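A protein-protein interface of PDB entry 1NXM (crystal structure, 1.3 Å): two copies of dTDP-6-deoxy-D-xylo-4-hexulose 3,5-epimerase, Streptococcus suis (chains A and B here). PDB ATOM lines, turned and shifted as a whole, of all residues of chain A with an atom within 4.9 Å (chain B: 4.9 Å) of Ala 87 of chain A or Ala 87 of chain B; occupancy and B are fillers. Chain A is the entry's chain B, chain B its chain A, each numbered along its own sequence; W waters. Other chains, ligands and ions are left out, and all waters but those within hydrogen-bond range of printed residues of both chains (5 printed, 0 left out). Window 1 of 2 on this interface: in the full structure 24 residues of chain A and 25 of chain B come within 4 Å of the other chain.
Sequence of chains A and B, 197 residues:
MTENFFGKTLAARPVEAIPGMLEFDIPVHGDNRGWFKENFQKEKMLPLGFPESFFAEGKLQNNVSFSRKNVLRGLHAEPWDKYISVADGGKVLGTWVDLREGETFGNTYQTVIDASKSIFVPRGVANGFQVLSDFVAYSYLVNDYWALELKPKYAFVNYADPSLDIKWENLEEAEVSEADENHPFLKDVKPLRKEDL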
ATOM      1  N   TRP A  35      -8.915 -14.741 -28.608  1.00  0.00           N
ATOM      2  CA  TRP A  35      -9.524 -14.548 -27.304  1.00  0.00           C
ATOM      3  C   TRP A  35     -10.367 -13.307 -27.272  1.00  0.00           C
ATOM      4  O   TRP A  35     -10.352 -12.503 -28.214  1.00  0.00           O
ATOM      5  CB  TRP A  35      -8.460 -14.533 -26.185  1.00  0.00           C
ATOM      6  CG  TRP A  35      -7.265 -13.662 -26.424  1.00  0.00           C
ATOM      7  CD1 TRP A  35      -6.005 -14.098 -26.753  1.00  0.00           C
ATOM      8  CD2 TRP A  35      -7.176 -12.236 -26.301  1.00  0.00           C
ATOM      9  NE1 TRP A  35      -5.152 -13.028 -26.855  1.00  0.00           N
ATOM     10  CE2 TRP A  35      -5.833 -11.876 -26.563  1.00  0.00           C
ATOM     11  CE3 TRP A  35      -8.079 -11.223 -25.975  1.00  0.00           C
ATOM     12  CZ2 TRP A  35      -5.384 -10.552 -26.529  1.00  0.00           C
ATOM     13  CZ3 TRP A  35      -7.639  -9.913 -25.995  1.00  0.00           C
ATOM     14  CH2 TRP A  35      -6.298  -9.591 -26.261  1.00  0.00           C
ATOM     15  N   LYS A  37     -12.075 -10.318 -24.261  1.00  0.00           N
ATOM     16  CA  LYS A  37     -12.191  -9.800 -22.905  1.00  0.00           C
ATOM     17  C   LYS A  37     -13.145  -8.607 -22.874  1.00  0.00           C
ATOM     18  O   LYS A  37     -13.290  -7.853 -23.841  1.00  0.00           O
ATOM     19  CB  LYS A  37     -10.831  -9.363 -22.345  1.00  0.00           C
ATOM     20  CG  LYS A  37     -10.113  -8.267 -23.110  1.00  0.00           C
ATOM     21  CD  LYS A  37      -8.992  -7.670 -22.309  1.00  0.00           C
ATOM     22  CE  LYS A  37      -8.129  -6.720 -23.104  1.00  0.00           C
ATOM     23  NZ  LYS A  37      -7.129  -6.031 -22.198  1.00  0.00           N
ATOM     24  N   VAL A  64      -4.445   5.079 -28.140  1.00  0.00           N
ATOM     25  CA  VAL A  64      -3.736   3.838 -28.417  1.00  0.00           C
ATOM     26  C   VAL A  64      -2.370   4.182 -28.963  1.00  0.00           C
ATOM     27  O   VAL A  64      -2.219   4.996 -29.872  1.00  0.00           O
ATOM     28  CB  VAL A  64      -4.504   2.973 -29.448  1.00  0.00           C
ATOM     29  CG1 VAL A  64      -3.763   1.700 -29.772  1.00  0.00           C
ATOM     30  CG2 VAL A  64      -5.924   2.624 -28.942  1.00  0.00           C
ATOM     31  N   PHE A  66       0.882   1.959 -30.609  1.00  0.00           N
ATOM     32  CA  PHE A  66       1.341   0.680 -31.138  1.00  0.00           C
ATOM     33  C   PHE A  66       2.841   0.815 -31.253  1.00  0.00           C
ATOM     34  O   PHE A  66       3.339   1.641 -31.993  1.00  0.00           O
ATOM     35  CB  PHE A  66       0.671   0.398 -32.504  1.00  0.00           C
ATOM     36  CG  PHE A  66       0.966  -0.979 -33.030  1.00  0.00           C
ATOM     37  CD1 PHE A  66       0.519  -2.105 -32.356  1.00  0.00           C
ATOM     38  CD2 PHE A  66       1.726  -1.151 -34.180  1.00  0.00           C
ATOM     39  CE1 PHE A  66       0.797  -3.371 -32.825  1.00  0.00           C
ATOM     40  CE2 PHE A  66       2.019  -2.437 -34.651  1.00  0.00           C
ATOM     41  CZ  PHE A  66       1.546  -3.532 -33.971  1.00  0.00           C
ATOM     42  N   SER A  85      -4.489  -0.550 -20.334  1.00  0.00           N
ATOM     43  CA  SER A  85      -4.305  -2.000 -20.585  1.00  0.00           C
ATOM     44  C   SER A  85      -3.713  -2.196 -21.961  1.00  0.00           C
ATOM     45  O   SER A  85      -3.295  -1.254 -22.638  1.00  0.00           O
ATOM     46  CB  SER A  85      -5.599  -2.869 -20.409  1.00  0.00           C
ATOM     47  OG  SER A  85      -5.374  -4.351 -20.377  1.00  0.00           O
ATOM     48  N   VAL A  86      -3.663  -3.456 -22.341  1.00  0.00           N
ATOM     49  CA  VAL A  86      -3.100  -3.900 -23.599  1.00  0.00           C
ATOM     50  C   VAL A  86      -4.218  -4.561 -24.397  1.00  0.00           C
ATOM     51  O   VAL A  86      -4.977  -5.360 -23.853  1.00  0.00           O
ATOM     52  CB  VAL A  86      -1.925  -4.843 -23.343  1.00  0.00           C
ATOM     53  CG1 VAL A  86      -1.524  -5.634 -24.561  1.00  0.00           C
ATOM     54  CG2 VAL A  86      -0.735  -4.034 -22.817  1.00  0.00           C
ATOM     55  N   ALA A  87      -4.296  -4.262 -25.693  1.00  0.00           N
ATOM     56  CA  ALA A  87      -5.387  -4.711 -26.549  1.00  0.00           C
ATOM     57  C   ALA A  87      -5.019  -5.850 -27.448  1.00  0.00           C
ATOM     58  O   ALA A  87      -5.899  -6.418 -28.039  1.00  0.00           O
ATOM     59  CB  ALA A  87      -5.934  -3.564 -27.387  1.00  0.00           C
ATOM     60  N   ASP A  88      -3.740  -6.188 -27.574  1.00  0.00           N
ATOM     61  CA  ASP A  88      -3.310  -7.297 -28.406  1.00  0.00           C
ATOM     62  C   ASP A  88      -2.592  -8.336 -27.574  1.00  0.00           C
ATOM     63  O   ASP A  88      -2.787  -8.391 -26.360  1.00  0.00           O
ATOM     64  CB  ASP A  88      -2.515  -6.826 -29.637  1.00  0.00           C
ATOM     65  CG  ASP A  88      -1.149  -6.276 -29.306  1.00  0.00           C
ATOM     66  OD1 ASP A  88      -0.810  -6.110 -28.098  1.00  0.00           O
ATOM     67  OD2 ASP A  88      -0.378  -5.980 -30.248  1.00  0.00           O
ATOM     68  N   GLY A  89      -1.797  -9.184 -28.219  1.00  0.00           N
ATOM     69  CA  GLY A  89      -1.037 -10.214 -27.530  1.00  0.00           C
ATOM     70  C   GLY A  89       0.276  -9.779 -26.912  1.00  0.00           C
ATOM     71  O   GLY A  89       1.011 -10.622 -26.429  1.00  0.00           O
ATOM     72  N   ALA A 137      -0.032  -3.236 -28.478  1.00  0.00           N
ATOM     73  CA  ALA A 137      -1.113  -2.260 -28.620  1.00  0.00           C
ATOM     74  C   ALA A 137      -1.525  -1.829 -27.214  1.00  0.00           C
ATOM     75  O   ALA A 137      -2.165  -2.571 -26.467  1.00  0.00           O
ATOM     76  CB  ALA A 137      -2.284  -2.871 -29.391  1.00  0.00           C
ATOM     77  N   SER A 139      -3.529   0.540 -24.913  1.00  0.00           N
ATOM     78  CA  SER A 139      -4.801   1.243 -25.055  1.00  0.00           C
ATOM     79  C   SER A 139      -5.242   1.768 -23.714  1.00  0.00           C
ATOM     80  O   SER A 139      -5.384   0.985 -22.775  1.00  0.00           O
ATOM     81  CB  SER A 139      -5.869   0.295 -25.618  1.00  0.00           C
ATOM     82  OG  SER A 139      -7.118   0.957 -25.823  1.00  0.00           O
ATOM     83  N   TRP B  35       3.217   3.814 -33.918  1.00  0.00           N
ATOM     84  CA  TRP B  35       2.353   4.975 -34.083  1.00  0.00           C
ATOM     85  C   TRP B  35       1.486   5.220 -32.876  1.00  0.00           C
ATOM     86  O   TRP B  35       1.466   4.434 -31.930  1.00  0.00           O
ATOM     87  CB  TRP B  35       1.514   4.826 -35.370  1.00  0.00           C
ATOM     88  CG  TRP B  35       0.852   3.479 -35.577  1.00  0.00           C
ATOM     89  CD1 TRP B  35       1.256   2.502 -36.466  1.00  0.00           C
ATOM     90  CD2 TRP B  35      -0.319   2.970 -34.935  1.00  0.00           C
ATOM     91  NE1 TRP B  35       0.412   1.423 -36.396  1.00  0.00           N
ATOM     92  CE2 TRP B  35      -0.563   1.685 -35.468  1.00  0.00           C
ATOM     93  CE3 TRP B  35      -1.169   3.434 -33.930  1.00  0.00           C
ATOM     94  CZ2 TRP B  35      -1.629   0.885 -35.032  1.00  0.00           C
ATOM     95  CZ3 TRP B  35      -2.227   2.637 -33.524  1.00  0.00           C
ATOM     96  CH2 TRP B  35      -2.435   1.382 -34.069  1.00  0.00           C
ATOM     97  N   LYS B  37      -2.531   7.158 -31.761  1.00  0.00           N
ATOM     98  CA  LYS B  37      -3.782   7.794 -32.145  1.00  0.00           C
ATOM     99  C   LYS B  37      -4.626   8.119 -30.934  1.00  0.00           C
ATOM    100  O   LYS B  37      -4.558   7.450 -29.910  1.00  0.00           O
ATOM    101  CB  LYS B  37      -4.589   6.898 -33.088  1.00  0.00           C
ATOM    102  CG  LYS B  37      -5.004   5.541 -32.534  1.00  0.00           C
ATOM    103  CD  LYS B  37      -6.066   4.902 -33.368  1.00  0.00           C
ATOM    104  CE  LYS B  37      -6.431   3.477 -33.030  1.00  0.00           C
ATOM    105  NZ  LYS B  37      -7.626   3.034 -33.796  1.00  0.00           N
ATOM    106  N   VAL B  64     -12.692  -6.166 -26.173  1.00  0.00           N
ATOM    107  CA  VAL B  64     -11.623  -6.399 -27.125  1.00  0.00           C
ATOM    108  C   VAL B  64     -11.618  -7.857 -27.527  1.00  0.00           C
ATOM    109  O   VAL B  64     -11.665  -8.736 -26.682  1.00  0.00           O
ATOM    110  CB  VAL B  64     -10.252  -6.041 -26.536  1.00  0.00           C
ATOM    111  CG1 VAL B  64      -9.183  -6.352 -27.559  1.00  0.00           C
ATOM    112  CG2 VAL B  64     -10.198  -4.596 -26.156  1.00  0.00           C
ATOM    113  N   PHE B  66      -9.248 -10.516 -29.964  1.00  0.00           N
ATOM    114  CA  PHE B  66      -8.003 -10.734 -30.686  1.00  0.00           C
ATOM    115  C   PHE B  66      -8.239 -11.971 -31.531  1.00  0.00           C
ATOM    116  O   PHE B  66      -8.494 -13.041 -30.998  1.00  0.00           O
ATOM    117  CB  PHE B  66      -6.854 -10.896 -29.705  1.00  0.00           C
ATOM    118  CG  PHE B  66      -5.520 -10.927 -30.370  1.00  0.00           C
ATOM    119  CD1 PHE B  66      -5.043  -9.816 -31.026  1.00  0.00           C
ATOM    120  CD2 PHE B  66      -4.779 -12.092 -30.405  1.00  0.00           C
ATOM    121  CE1 PHE B  66      -3.807  -9.845 -31.665  1.00  0.00           C
ATOM    122  CE2 PHE B  66      -3.556 -12.122 -31.038  1.00  0.00           C
ATOM    123  CZ  PHE B  66      -3.094 -10.989 -31.677  1.00  0.00           C
ATOM    124  N   SER B  85     -13.487  -0.085 -33.532  1.00  0.00           N
ATOM    125  CA  SER B  85     -12.174   0.335 -33.948  1.00  0.00           C
ATOM    126  C   SER B  85     -11.206  -0.839 -33.958  1.00  0.00           C
ATOM    127  O   SER B  85     -11.511  -1.916 -33.452  1.00  0.00           O
ATOM    128  CB  SER B  85     -11.674   1.407 -33.019  1.00  0.00           C
ATOM    129  OG  SER B  85     -11.393   0.953 -31.707  1.00  0.00           O
ATOM    130  N   VAL B  86     -10.017  -0.592 -34.501  1.00  0.00           N
ATOM    131  CA  VAL B  86      -8.909  -1.519 -34.468  1.00  0.00           C
ATOM    132  C   VAL B  86      -7.742  -0.900 -33.711  1.00  0.00           C
ATOM    133  O   VAL B  86      -7.366   0.243 -33.969  1.00  0.00           O
ATOM    134  CB  VAL B  86      -8.507  -1.924 -35.888  1.00  0.00           C
ATOM    135  CG1 VAL B  86      -7.163  -2.612 -35.932  1.00  0.00           C
ATOM    136  CG2 VAL B  86      -9.573  -2.809 -36.474  1.00  0.00           C
ATOM    137  N   ALA B  87      -7.199  -1.650 -32.754  1.00  0.00           N
ATOM    138  CA  ALA B  87      -6.185  -1.149 -31.835  1.00  0.00           C
ATOM    139  C   ALA B  87      -4.757  -1.499 -32.202  1.00  0.00           C
ATOM    140  O   ALA B  87      -3.845  -0.948 -31.631  1.00  0.00           O
ATOM    141  CB  ALA B  87      -6.478  -1.600 -30.444  1.00  0.00           C
ATOM    142  N   ASP B  88      -4.560  -2.428 -33.136  1.00  0.00           N
ATOM    143  CA  ASP B  88      -3.240  -2.806 -33.562  1.00  0.00           C
ATOM    144  C   ASP B  88      -3.050  -2.513 -35.036  1.00  0.00           C
ATOM    145  O   ASP B  88      -3.760  -1.696 -35.608  1.00  0.00           O
ATOM    146  CB  ASP B  88      -2.898  -4.242 -33.161  1.00  0.00           C
ATOM    147  CG  ASP B  88      -3.655  -5.289 -33.926  1.00  0.00           C
ATOM    148  OD1 ASP B  88      -4.575  -4.937 -34.690  1.00  0.00           O
ATOM    149  OD2 ASP B  88      -3.345  -6.507 -33.764  1.00  0.00           O
ATOM    150  N   GLY B  89      -2.072  -3.157 -35.658  1.00  0.00           N
ATOM    151  CA  GLY B  89      -1.795  -2.933 -37.058  1.00  0.00           C
ATOM    152  C   GLY B  89      -2.625  -3.772 -38.013  1.00  0.00           C
ATOM    153  O   GLY B  89      -2.345  -3.808 -39.206  1.00  0.00           O
ATOM    154  N   ALA B 137      -6.569  -6.790 -33.385  1.00  0.00           N
ATOM    155  CA  ALA B 137      -7.109  -6.397 -32.098  1.00  0.00           C
ATOM    156  C   ALA B 137      -8.298  -5.490 -32.372  1.00  0.00           C
ATOM    157  O   ALA B 137      -8.146  -4.354 -32.829  1.00  0.00           O
ATOM    158  CB  ALA B 137      -6.069  -5.686 -31.260  1.00  0.00           C
ATOM    159  N   SER B 139     -11.396  -3.525 -31.019  1.00  0.00           N
ATOM    160  CA  SER B 139     -11.702  -2.855 -29.770  1.00  0.00           C
ATOM    161  C   SER B 139     -12.916  -1.987 -29.943  1.00  0.00           C
ATOM    162  O   SER B 139     -12.918  -1.092 -30.808  1.00  0.00           O
ATOM    163  CB  SER B 139     -10.531  -1.983 -29.315  1.00  0.00           C
ATOM    164  OG  SER B 139     -10.825  -1.300 -28.098  1.00  0.00           O
HETATM  165  O   HOH W   1       4.042   4.681 -30.645  1.00  0.00           O
HETATM  166  O   HOH W   2     -11.637 -13.910 -30.555  1.00  0.00           O
HETATM  167  O   HOH W   3      -9.032   0.908 -28.077  1.00  0.00           O
HETATM  168  O   HOH W   4      -0.937  -7.087 -32.658  1.00  0.00           O
HETATM  169  O   HOH W   5      -9.000  -1.032 -25.512  1.00  0.00           O
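The backbone carbonyl oxygen (O) of Trp 35 of chain B lies within hydrogen-bond range of the backbone NH (N) of Phe 66 of chain A (2.9 Å).
The backbone NH of Phe 66 of chain B lies within hydrogen-bond range of the backbone carbonyl oxygen of Trp 35 of chain A (2.9 Å).
The backbone carbonyl oxygen (O) of Val 64 of chain B lies within hydrogen-bond range of the backbone NH (N) of Lys 37 of chain A (2.9 Å).
N of Lys 37 of chain B lies within hydrogen-bond range of O of Val 64 of chain A (2.9 Å).
The side-chain amino group of Lys 37 of chain A lies within hydrogen-bond range of the backbone carbonyl oxygen of Val 86 of chain A, 2.8 Å away.
The backbone NH of Ala 137 of chain B is in hydrogen-bond range of the side-chain carboxylate of Asp 88 of chain B (3.0 Å).
The side-chain amino group (NZ) of Lys 37 of chain A is in hydrogen-bond range of the side-chain hydroxyl (OG) of Ser 85 of chain A.
The backbone NH (N) of Ala 87 of chain A lies within hydrogen-bond range of the backbone carbonyl oxygen (O) of Ala 137 of chain A, at 2.8 Å.
N of Ala 137 of chain A sits at hydrogen-bond distance from OD1 of Asp 88 of chain A.
The side-chain amino group (NZ) of Lys 37 of chain B sits at hydrogen-bond distance from the backbone carbonyl oxygen (O) of Val 86 of chain B, 2.8 Å away.
Val 64 of chain A touches Ala 87 of chain B.
CB of Asp 88 of chain B touches CE1 of Phe 66 of chain A, at 3.8 Å.
Ala 87 of chain A touches Val 64 of chain B.
CB of Ala 87 of chain A touches CB of Ala 87 of chain B, at 3.7 Å.
O of Ala 87 of chain A touches CB of Ala 137 of chain B (3.3 Å).
Asp 88 of chain A touches Phe 66 of chain B (CB to CE1, 3.9 Å).
Ala 87 of chain B touches Ala 137 of chain A (O to CB, 3.3 Å).
Of the printed residues of chain B, Trp 35 of chain A touches Phe 66.
Of chain B, only Val 64, Ala 87 and Ala 137 come within 4 Å of Ala 87 of chain A.
Printed residues of chain B within 4 Å of Asp 88 of chain A: Phe 66.
Of the printed residues of chain A, Trp 35 of chain B touches Phe 66.
Of the printed residues of chain A, Lys 37 of chain B touches Val 64 (2.9 Å).
The nearest residue of chain B that does not touch Ala 87 of chain A is Phe 66 of chain B (4.6 Å).
The nearest residue of chain A that does not touch Ala 87 of chain B is Phe 66 of chain A (4.6 Å).
The nearest printed residue of chain B that does not touch Val 64 of chain A is Trp 35 of chain B (4.2 Å).
Of the 11 printed residues of chain B, 7 touch a printed residue of chain A.
Hydrophobic or aromatic side chains of chain A within 4 Å of the printed part of chain B: Trp 35, Val 64, Phe 66, Ala 87 and Ala 137.
Trp 35 of chain A touches Phe 66 of chain B, and with the chains exchanged Phe 66 of chain A touches Trp 35 of chain B.
Lys 37 of chain A touches Val 64 of chain B, and with the chains exchanged Val 64 of chain A touches Lys 37 of chain B.
Phe 66 of chain A touches Asp 88 of chain B, and with the chains exchanged Asp 88 of chain A touches Phe 66 of chain B.
Ala 87 of chain A touches Ala 137 of chain B, and with the chains exchanged Ala 137 of chain A touches Ala 87 of chain B.
Of the 11 pairs that touch across the chains among the printed residues, 11 have their exchanged pair printed and touching as well.
Water W4 lies within hydrogen-bond range of OD2 of Asp 88 of chain A (2.7 Å) and OD2 of Asp 88 of chain B (2.7 Å).
Water W5 lies within hydrogen-bond range of the side-chain hydroxyl of Ser 139 of chain A (2.8 Å) and the side-chain hydroxyl of Ser 139 of chain B (3.2 Å).
Water W3 bridges OG of Ser 139 of chain B and OG of Ser 139 of chain A.
Water W1 bridges O of Trp 35 of chain B and O of Phe 66 of chain A.
Water W2 bridges O of Trp 35 of chain A (3.0 Å) and O of Phe 66 of chain B (3.3 Å).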
